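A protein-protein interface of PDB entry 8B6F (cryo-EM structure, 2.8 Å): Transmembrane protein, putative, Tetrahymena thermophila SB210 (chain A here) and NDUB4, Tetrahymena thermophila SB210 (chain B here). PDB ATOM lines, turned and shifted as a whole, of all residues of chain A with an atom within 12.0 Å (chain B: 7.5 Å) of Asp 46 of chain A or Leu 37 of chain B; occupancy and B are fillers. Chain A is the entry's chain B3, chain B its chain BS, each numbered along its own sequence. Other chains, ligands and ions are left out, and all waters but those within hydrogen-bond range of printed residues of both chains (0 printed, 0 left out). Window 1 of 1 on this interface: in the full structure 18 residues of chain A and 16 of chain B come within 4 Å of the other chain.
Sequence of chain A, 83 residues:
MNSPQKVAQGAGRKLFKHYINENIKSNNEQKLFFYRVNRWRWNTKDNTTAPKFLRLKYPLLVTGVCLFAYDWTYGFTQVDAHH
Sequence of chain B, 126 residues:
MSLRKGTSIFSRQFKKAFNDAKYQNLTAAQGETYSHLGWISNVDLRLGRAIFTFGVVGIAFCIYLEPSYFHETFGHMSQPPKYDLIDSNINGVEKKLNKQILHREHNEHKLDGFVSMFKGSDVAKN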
ATOM      1  N   ASN A  38      10.958  -0.607  12.892  1.00  0.00           N
ATOM      2  CA  ASN A  38       9.774  -0.484  12.052  1.00  0.00           C
ATOM      3  C   ASN A  38       9.951   0.463  10.869  1.00  0.00           C
ATOM      4  O   ASN A  38       9.010   0.622  10.086  1.00  0.00           O
ATOM      5  CB  ASN A  38       8.584  -0.009  12.894  1.00  0.00           C
ATOM      6  CG  ASN A  38       8.048  -1.087  13.811  1.00  0.00           C
ATOM      7  OD1 ASN A  38       7.306  -1.967  13.382  1.00  0.00           O
ATOM      8  ND2 ASN A  38       8.406  -1.011  15.087  1.00  0.00           N
ATOM      9  N   ARG A  39      11.118   1.092  10.711  1.00  0.00           N
ATOM     10  CA  ARG A  39      11.289   2.063   9.631  1.00  0.00           C
ATOM     11  C   ARG A  39      10.906   1.486   8.274  1.00  0.00           C
ATOM     12  O   ARG A  39      10.313   2.181   7.442  1.00  0.00           O
ATOM     13  CB  ARG A  39      12.729   2.580   9.599  1.00  0.00           C
ATOM     14  CG  ARG A  39      13.070   3.489  10.766  1.00  0.00           C
ATOM     15  CD  ARG A  39      13.950   4.650  10.340  1.00  0.00           C
ATOM     16  NE  ARG A  39      14.222   5.555  11.449  1.00  0.00           N
ATOM     17  CZ  ARG A  39      15.267   5.468  12.260  1.00  0.00           C
ATOM     18  NH1 ARG A  39      16.182   4.523  12.113  1.00  0.00           N
ATOM     19  NH2 ARG A  39      15.398   6.351  13.245  1.00  0.00           N
ATOM     20  N   TRP A  40      11.235   0.218   8.028  1.00  0.00           N
ATOM     21  CA  TRP A  40      11.007  -0.360   6.709  1.00  0.00           C
ATOM     22  C   TRP A  40       9.536  -0.356   6.314  1.00  0.00           C
ATOM     23  O   TRP A  40       9.229  -0.369   5.117  1.00  0.00           O
ATOM     24  CB  TRP A  40      11.541  -1.793   6.671  1.00  0.00           C
ATOM     25  CG  TRP A  40      10.756  -2.742   7.508  1.00  0.00           C
ATOM     26  CD1 TRP A  40      10.982  -3.064   8.811  1.00  0.00           C
ATOM     27  CD2 TRP A  40       9.611  -3.497   7.099  1.00  0.00           C
ATOM     28  NE1 TRP A  40      10.048  -3.974   9.242  1.00  0.00           N
ATOM     29  CE2 TRP A  40       9.193  -4.255   8.209  1.00  0.00           C
ATOM     30  CE3 TRP A  40       8.896  -3.602   5.902  1.00  0.00           C
ATOM     31  CZ2 TRP A  40       8.096  -5.109   8.158  1.00  0.00           C
ATOM     32  CZ3 TRP A  40       7.807  -4.450   5.851  1.00  0.00           C
ATOM     33  CH2 TRP A  40       7.415  -5.192   6.973  1.00  0.00           C
ATOM     34  N   ARG A  41       8.622  -0.334   7.286  1.00  0.00           N
ATOM     35  CA  ARG A  41       7.207  -0.506   6.972  1.00  0.00           C
ATOM     36  C   ARG A  41       6.683   0.619   6.091  1.00  0.00           C
ATOM     37  O   ARG A  41       5.910   0.377   5.158  1.00  0.00           O
ATOM     38  CB  ARG A  41       6.393  -0.593   8.261  1.00  0.00           C
ATOM     39  CG  ARG A  41       6.656  -1.850   9.062  1.00  0.00           C
ATOM     40  CD  ARG A  41       5.703  -1.970  10.233  1.00  0.00           C
ATOM     41  NE  ARG A  41       5.865  -3.246  10.917  1.00  0.00           N
ATOM     42  CZ  ARG A  41       5.343  -4.391  10.498  1.00  0.00           C
ATOM     43  NH1 ARG A  41       4.625  -4.458   9.390  1.00  0.00           N
ATOM     44  NH2 ARG A  41       5.555  -5.497  11.202  1.00  0.00           N
ATOM     45  N   TRP A  42       7.088   1.858   6.369  1.00  0.00           N
ATOM     46  CA  TRP A  42       6.517   3.028   5.713  1.00  0.00           C
ATOM     47  C   TRP A  42       7.372   3.520   4.551  1.00  0.00           C
ATOM     48  O   TRP A  42       7.420   4.725   4.282  1.00  0.00           O
ATOM     49  CB  TRP A  42       6.309   4.143   6.735  1.00  0.00           C
ATOM     50  CG  TRP A  42       5.838   3.622   8.051  1.00  0.00           C
ATOM     51  CD1 TRP A  42       4.593   3.145   8.350  1.00  0.00           C
ATOM     52  CD2 TRP A  42       6.609   3.512   9.248  1.00  0.00           C
ATOM     53  NE1 TRP A  42       4.544   2.749   9.664  1.00  0.00           N
ATOM     54  CE2 TRP A  42       5.770   2.964  10.237  1.00  0.00           C
ATOM     55  CE3 TRP A  42       7.928   3.826   9.581  1.00  0.00           C
ATOM     56  CZ2 TRP A  42       6.208   2.725  11.535  1.00  0.00           C
ATOM     57  CZ3 TRP A  42       8.362   3.589  10.869  1.00  0.00           C
ATOM     58  CH2 TRP A  42       7.505   3.044  11.832  1.00  0.00           C
ATOM     59  N   ASN A  43       8.047   2.611   3.854  1.00  0.00           N
ATOM     60  CA  ASN A  43       8.820   2.997   2.683  1.00  0.00           C
ATOM     61  C   ASN A  43       7.894   3.551   1.609  1.00  0.00           C
ATOM     62  O   ASN A  43       6.894   2.924   1.250  1.00  0.00           O
ATOM     63  CB  ASN A  43       9.594   1.791   2.151  1.00  0.00           C
ATOM     64  CG  ASN A  43      10.565   2.157   1.047  1.00  0.00           C
ATOM     65  OD1 ASN A  43      10.414   3.181   0.384  1.00  0.00           O
ATOM     66  ND2 ASN A  43      11.568   1.313   0.842  1.00  0.00           N
ATOM     67  N   THR A  44       8.231   4.734   1.095  1.00  0.00           N
ATOM     68  CA  THR A  44       7.419   5.345   0.050  1.00  0.00           C
ATOM     69  C   THR A  44       7.631   4.677  -1.302  1.00  0.00           C
ATOM     70  O   THR A  44       6.733   4.708  -2.149  1.00  0.00           O
ATOM     71  CB  THR A  44       7.724   6.840  -0.049  1.00  0.00           C
ATOM     72  OG1 THR A  44       9.142   7.040  -0.108  1.00  0.00           O
ATOM     73  CG2 THR A  44       7.155   7.578   1.152  1.00  0.00           C
ATOM     74  N   LYS A  45       8.800   4.076  -1.521  1.00  0.00           N
ATOM     75  CA  LYS A  45       9.070   3.367  -2.765  1.00  0.00           C
ATOM     76  C   LYS A  45       8.253   2.091  -2.911  1.00  0.00           C
ATOM     77  O   LYS A  45       8.213   1.528  -4.009  1.00  0.00           O
ATOM     78  CB  LYS A  45      10.558   3.020  -2.860  1.00  0.00           C
ATOM     79  CG  LYS A  45      11.440   4.173  -3.302  1.00  0.00           C
ATOM     80  CD  LYS A  45      12.916   3.803  -3.287  1.00  0.00           C
ATOM     81  CE  LYS A  45      13.438   3.625  -1.870  1.00  0.00           C
ATOM     82  NZ  LYS A  45      14.903   3.357  -1.850  1.00  0.00           N
ATOM     83  N   ASP A  46       7.603   1.624  -1.844  1.00  0.00           N
ATOM     84  CA  ASP A  46       6.958   0.322  -1.844  1.00  0.00           C
ATOM     85  C   ASP A  46       5.442   0.377  -1.711  1.00  0.00           C
ATOM     86  O   ASP A  46       4.788  -0.649  -1.923  1.00  0.00           O
ATOM     87  CB  ASP A  46       7.526  -0.539  -0.705  1.00  0.00           C
ATOM     88  CG  ASP A  46       7.223  -2.015  -0.878  1.00  0.00           C
ATOM     89  OD1 ASP A  46       6.749  -2.404  -1.965  1.00  0.00           O
ATOM     90  OD2 ASP A  46       7.461  -2.787   0.073  1.00  0.00           O
ATOM     91  N   ASN A  47       4.864   1.525  -1.363  1.00  0.00           N
ATOM     92  CA  ASN A  47       3.426   1.622  -1.150  1.00  0.00           C
ATOM     93  C   ASN A  47       2.881   2.874  -1.825  1.00  0.00           C
ATOM     94  O   ASN A  47       3.573   3.889  -1.936  1.00  0.00           O
ATOM     95  CB  ASN A  47       3.085   1.637   0.344  1.00  0.00           C
ATOM     96  CG  ASN A  47       1.634   1.304   0.610  1.00  0.00           C
ATOM     97  OD1 ASN A  47       0.761   1.594  -0.205  1.00  0.00           O
ATOM     98  ND2 ASN A  47       1.370   0.680   1.751  1.00  0.00           N
ATOM     99  N   THR A  48       1.628   2.790  -2.272  1.00  0.00           N
ATOM    100  CA  THR A  48       0.943   3.907  -2.913  1.00  0.00           C
ATOM    101  C   THR A  48      -0.518   3.873  -2.472  1.00  0.00           C
ATOM    102  O   THR A  48      -0.886   3.160  -1.534  1.00  0.00           O
ATOM    103  CB  THR A  48       1.092   3.846  -4.442  1.00  0.00           C
ATOM    104  OG1 THR A  48       0.783   5.127  -5.004  1.00  0.00           O
ATOM    105  CG2 THR A  48       0.138   2.828  -5.057  1.00  0.00           C
ATOM    106  N   THR A  49      -1.356   4.646  -3.153  1.00  0.00           N
ATOM    107  CA  THR A  49      -2.773   4.740  -2.847  1.00  0.00           C
ATOM    108  C   THR A  49      -3.592   4.101  -3.962  1.00  0.00           C
ATOM    109  O   THR A  49      -3.150   3.991  -5.107  1.00  0.00           O
ATOM    110  CB  THR A  49      -3.204   6.198  -2.657  1.00  0.00           C
ATOM    111  OG1 THR A  49      -3.228   6.865  -3.925  1.00  0.00           O
ATOM    112  CG2 THR A  49      -2.241   6.921  -1.734  1.00  0.00           C
ATOM    113  N   ALA A  50      -4.805   3.684  -3.607  1.00  0.00           N
ATOM    114  CA  ALA A  50      -5.680   3.039  -4.582  1.00  0.00           C
ATOM    115  C   ALA A  50      -5.991   3.929  -5.777  1.00  0.00           C
ATOM    116  O   ALA A  50      -5.945   3.424  -6.913  1.00  0.00           O
ATOM    117  CB  ALA A  50      -6.970   2.580  -3.894  1.00  0.00           C
ATOM    118  N   LYS A  52      -4.090   6.149  -7.129  1.00  0.00           N
ATOM    119  CA  LYS A  52      -2.881   6.168  -7.948  1.00  0.00           C
ATOM    120  C   LYS A  52      -2.700   4.858  -8.705  1.00  0.00           C
ATOM    121  O   LYS A  52      -2.302   4.865  -9.875  1.00  0.00           O
ATOM    122  CB  LYS A  52      -1.659   6.446  -7.076  1.00  0.00           C
ATOM    123  CG  LYS A  52      -1.571   7.865  -6.535  1.00  0.00           C
ATOM    124  CD  LYS A  52      -0.155   8.163  -6.061  1.00  0.00           C
ATOM    125  CE  LYS A  52      -0.088   9.413  -5.208  1.00  0.00           C
ATOM    126  NZ  LYS A  52      -0.673   9.188  -3.861  1.00  0.00           N
ATOM    127  N   PHE A  53      -2.971   3.725  -8.057  1.00  0.00           N
ATOM    128  CA  PHE A  53      -2.751   2.438  -8.711  1.00  0.00           C
ATOM    129  C   PHE A  53      -3.798   2.172  -9.786  1.00  0.00           C
ATOM    130  O   PHE A  53      -3.472   1.657 -10.861  1.00  0.00           O
ATOM    131  CB  PHE A  53      -2.754   1.312  -7.679  1.00  0.00           C
ATOM    132  CG  PHE A  53      -2.439  -0.038  -8.259  1.00  0.00           C
ATOM    133  CD1 PHE A  53      -1.150  -0.351  -8.654  1.00  0.00           C
ATOM    134  CD2 PHE A  53      -3.430  -0.993  -8.405  1.00  0.00           C
ATOM    135  CE1 PHE A  53      -0.856  -1.592  -9.186  1.00  0.00           C
ATOM    136  CE2 PHE A  53      -3.145  -2.234  -8.936  1.00  0.00           C
ATOM    137  CZ  PHE A  53      -1.855  -2.534  -9.326  1.00  0.00           C
ATOM    138  N   TYR B  34      17.682  -3.015   1.466  1.00  0.00           N
ATOM    139  CA  TYR B  34      16.636  -2.265   0.783  1.00  0.00           C
ATOM    140  C   TYR B  34      15.320  -3.010   0.933  1.00  0.00           C
ATOM    141  O   TYR B  34      15.284  -4.242   0.877  1.00  0.00           O
ATOM    142  CB  TYR B  34      16.966  -2.060  -0.699  1.00  0.00           C
ATOM    143  CG  TYR B  34      17.265  -3.339  -1.439  1.00  0.00           C
ATOM    144  CD1 TYR B  34      16.249  -4.076  -2.031  1.00  0.00           C
ATOM    145  CD2 TYR B  34      18.564  -3.809  -1.549  1.00  0.00           C
ATOM    146  CE1 TYR B  34      16.520  -5.247  -2.708  1.00  0.00           C
ATOM    147  CE2 TYR B  34      18.845  -4.977  -2.224  1.00  0.00           C
ATOM    148  CZ  TYR B  34      17.820  -5.690  -2.801  1.00  0.00           C
ATOM    149  OH  TYR B  34      18.100  -6.855  -3.475  1.00  0.00           O
ATOM    150  N   SER B  35      14.240  -2.257   1.131  1.00  0.00           N
ATOM    151  CA  SER B  35      12.928  -2.832   1.392  1.00  0.00           C
ATOM    152  C   SER B  35      11.973  -2.755   0.213  1.00  0.00           C
ATOM    153  O   SER B  35      11.073  -3.590   0.113  1.00  0.00           O
ATOM    154  CB  SER B  35      12.278  -2.123   2.588  1.00  0.00           C
ATOM    155  OG  SER B  35      13.145  -2.139   3.707  1.00  0.00           O
ATOM    156  N   HIS B  36      12.144  -1.783  -0.675  1.00  0.00           N
ATOM    157  CA  HIS B  36      11.199  -1.582  -1.761  1.00  0.00           C
ATOM    158  C   HIS B  36      11.351  -2.663  -2.827  1.00  0.00           C
ATOM    159  O   HIS B  36      12.396  -3.301  -2.965  1.00  0.00           O
ATOM    160  CB  HIS B  36      11.399  -0.209  -2.397  1.00  0.00           C
ATOM    161  CG  HIS B  36      12.668  -0.089  -3.179  1.00  0.00           C
ATOM    162  ND1 HIS B  36      13.880   0.198  -2.591  1.00  0.00           N
ATOM    163  CD2 HIS B  36      12.914  -0.223  -4.504  1.00  0.00           C
ATOM    164  CE1 HIS B  36      14.819   0.236  -3.520  1.00  0.00           C
ATOM    165  NE2 HIS B  36      14.260  -0.016  -4.689  1.00  0.00           N
ATOM    166  N   LEU B  37      10.275  -2.865  -3.581  1.00  0.00           N
ATOM    167  CA  LEU B  37      10.288  -3.693  -4.778  1.00  0.00           C
ATOM    168  C   LEU B  37      10.492  -2.774  -5.976  1.00  0.00           C
ATOM    169  O   LEU B  37       9.726  -1.824  -6.169  1.00  0.00           O
ATOM    170  CB  LEU B  37       8.987  -4.485  -4.908  1.00  0.00           C
ATOM    171  CG  LEU B  37       8.835  -5.377  -6.143  1.00  0.00           C
ATOM    172  CD1 LEU B  37       9.831  -6.519  -6.127  1.00  0.00           C
ATOM    173  CD2 LEU B  37       7.418  -5.911  -6.228  1.00  0.00           C
ATOM    174  N   GLY B  38      11.518  -3.053  -6.772  1.00  0.00           N
ATOM    175  CA  GLY B  38      11.909  -2.170  -7.849  1.00  0.00           C
ATOM    176  C   GLY B  38      11.150  -2.330  -9.143  1.00  0.00           C
ATOM    177  O   GLY B  38      11.491  -1.679 -10.132  1.00  0.00           O
ATOM    178  N   TRP B  39      10.129  -3.179  -9.173  1.00  0.00           N
ATOM    179  CA  TRP B  39       9.393  -3.461 -10.396  1.00  0.00           C
ATOM    180  C   TRP B  39       8.034  -4.028 -10.013  1.00  0.00           C
ATOM    181  O   TRP B  39       7.693  -4.132  -8.832  1.00  0.00           O
ATOM    182  CB  TRP B  39      10.170  -4.433 -11.286  1.00  0.00           C
ATOM    183  CG  TRP B  39      10.394  -5.750 -10.619  1.00  0.00           C
ATOM    184  CD1 TRP B  39       9.659  -6.884 -10.780  1.00  0.00           C
ATOM    185  CD2 TRP B  39      11.415  -6.064  -9.664  1.00  0.00           C
ATOM    186  NE1 TRP B  39      10.162  -7.888  -9.991  1.00  0.00           N
ATOM    187  CE2 TRP B  39      11.240  -7.409  -9.296  1.00  0.00           C
ATOM    188  CE3 TRP B  39      12.463  -5.338  -9.090  1.00  0.00           C
ATOM    189  CZ2 TRP B  39      12.072  -8.046  -8.380  1.00  0.00           C
ATOM    190  CZ3 TRP B  39      13.286  -5.970  -8.181  1.00  0.00           C
ATOM    191  CH2 TRP B  39      13.087  -7.312  -7.834  1.00  0.00           C
ATOM    192  N   ILE B  40       7.259  -4.398 -11.026  1.00  0.00           N
ATOM    193  CA  ILE B  40       5.969  -5.047 -10.832  1.00  0.00           C
ATOM    194  C   ILE B  40       5.865  -6.177 -11.845  1.00  0.00           C
ATOM    195  O   ILE B  40       6.293  -6.036 -12.994  1.00  0.00           O
ATOM    196  CB  ILE B  40       4.797  -4.056 -10.984  1.00  0.00           C
ATOM    197  CG1 ILE B  40       5.031  -2.834 -10.088  1.00  0.00           C
ATOM    198  CG2 ILE B  40       3.483  -4.745 -10.646  1.00  0.00           C
ATOM    199  CD1 ILE B  40       3.872  -1.847 -10.028  1.00  0.00           C
ATOM    200  N   SER B  41       5.310  -7.304 -11.410  1.00  0.00           N
ATOM    201  CA  SER B  41       5.153  -8.461 -12.282  1.00  0.00           C
ATOM    202  C   SER B  41       4.512  -8.058 -13.601  1.00  0.00           C
ATOM    203  O   SER B  41       3.380  -7.569 -13.630  1.00  0.00           O
ATOM    204  CB  SER B  41       4.313  -9.527 -11.580  1.00  0.00           C
ATOM    205  OG  SER B  41       4.037 -10.605 -12.454  1.00  0.00           O
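The side-chain amide nitrogen of Asn 43 of chain A sits close to the backbone NH of His 36 of chain B.
ND1 of His 36 of chain B lies within hydrogen-bond range of NZ of Lys 45 of chain A (3.4 Å).
OD1 of Asn 43 of chain A is in hydrogen-bond range of N of Lys 45 of chain A (2.7 Å).
Among the printed residues, merely in contact across the chains: Trp 40 of chain A with Ser 35 of chain B (3.4 Å), Asp 46 of chain A with Ser 35 of chain B (3.7 Å), Asp 46 of chain A with Leu 37 of chain B (3.9 Å), Asn 43 of chain A with Ser 35 of chain B (3.9 Å) and Asp 46 of chain A with His 36 of chain B (3.96 Å).
Asp 46 of chain A touches three residues of chain B.
Of chain A, only Asp 46 comes within 4 Å of Leu 37 of chain B.
Of the printed residues of chain A, His 36 of chain B touches Asn 43, Lys 45 and Asp 46.
No residue of chain A comes within 4 Å of Trp 39 of chain B.
Ile 40 of chain B touches none of the printed residues of chain A.
Printed residues of chain B within 4 Å of Asn 43 of chain A: Ser 35 and His 36.
Of the printed residues of chain B, Lys 45 of chain A touches His 36.
Of the printed residues of chain B, Trp 40 of chain A touches Ser 35.
Thr 44 of chain A touches none of the printed residues of chain B.
Of the 15 printed residues of chain A, 4 touch a printed residue of chain B.
Printed residues of chain A that touch a printed residue of chain B: Trp 40, Asn 43, Lys 45 and Asp 46.
Hydrophobic or aromatic side chains of chain A within 4 Å of the printed part of chain B: Trp 40.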
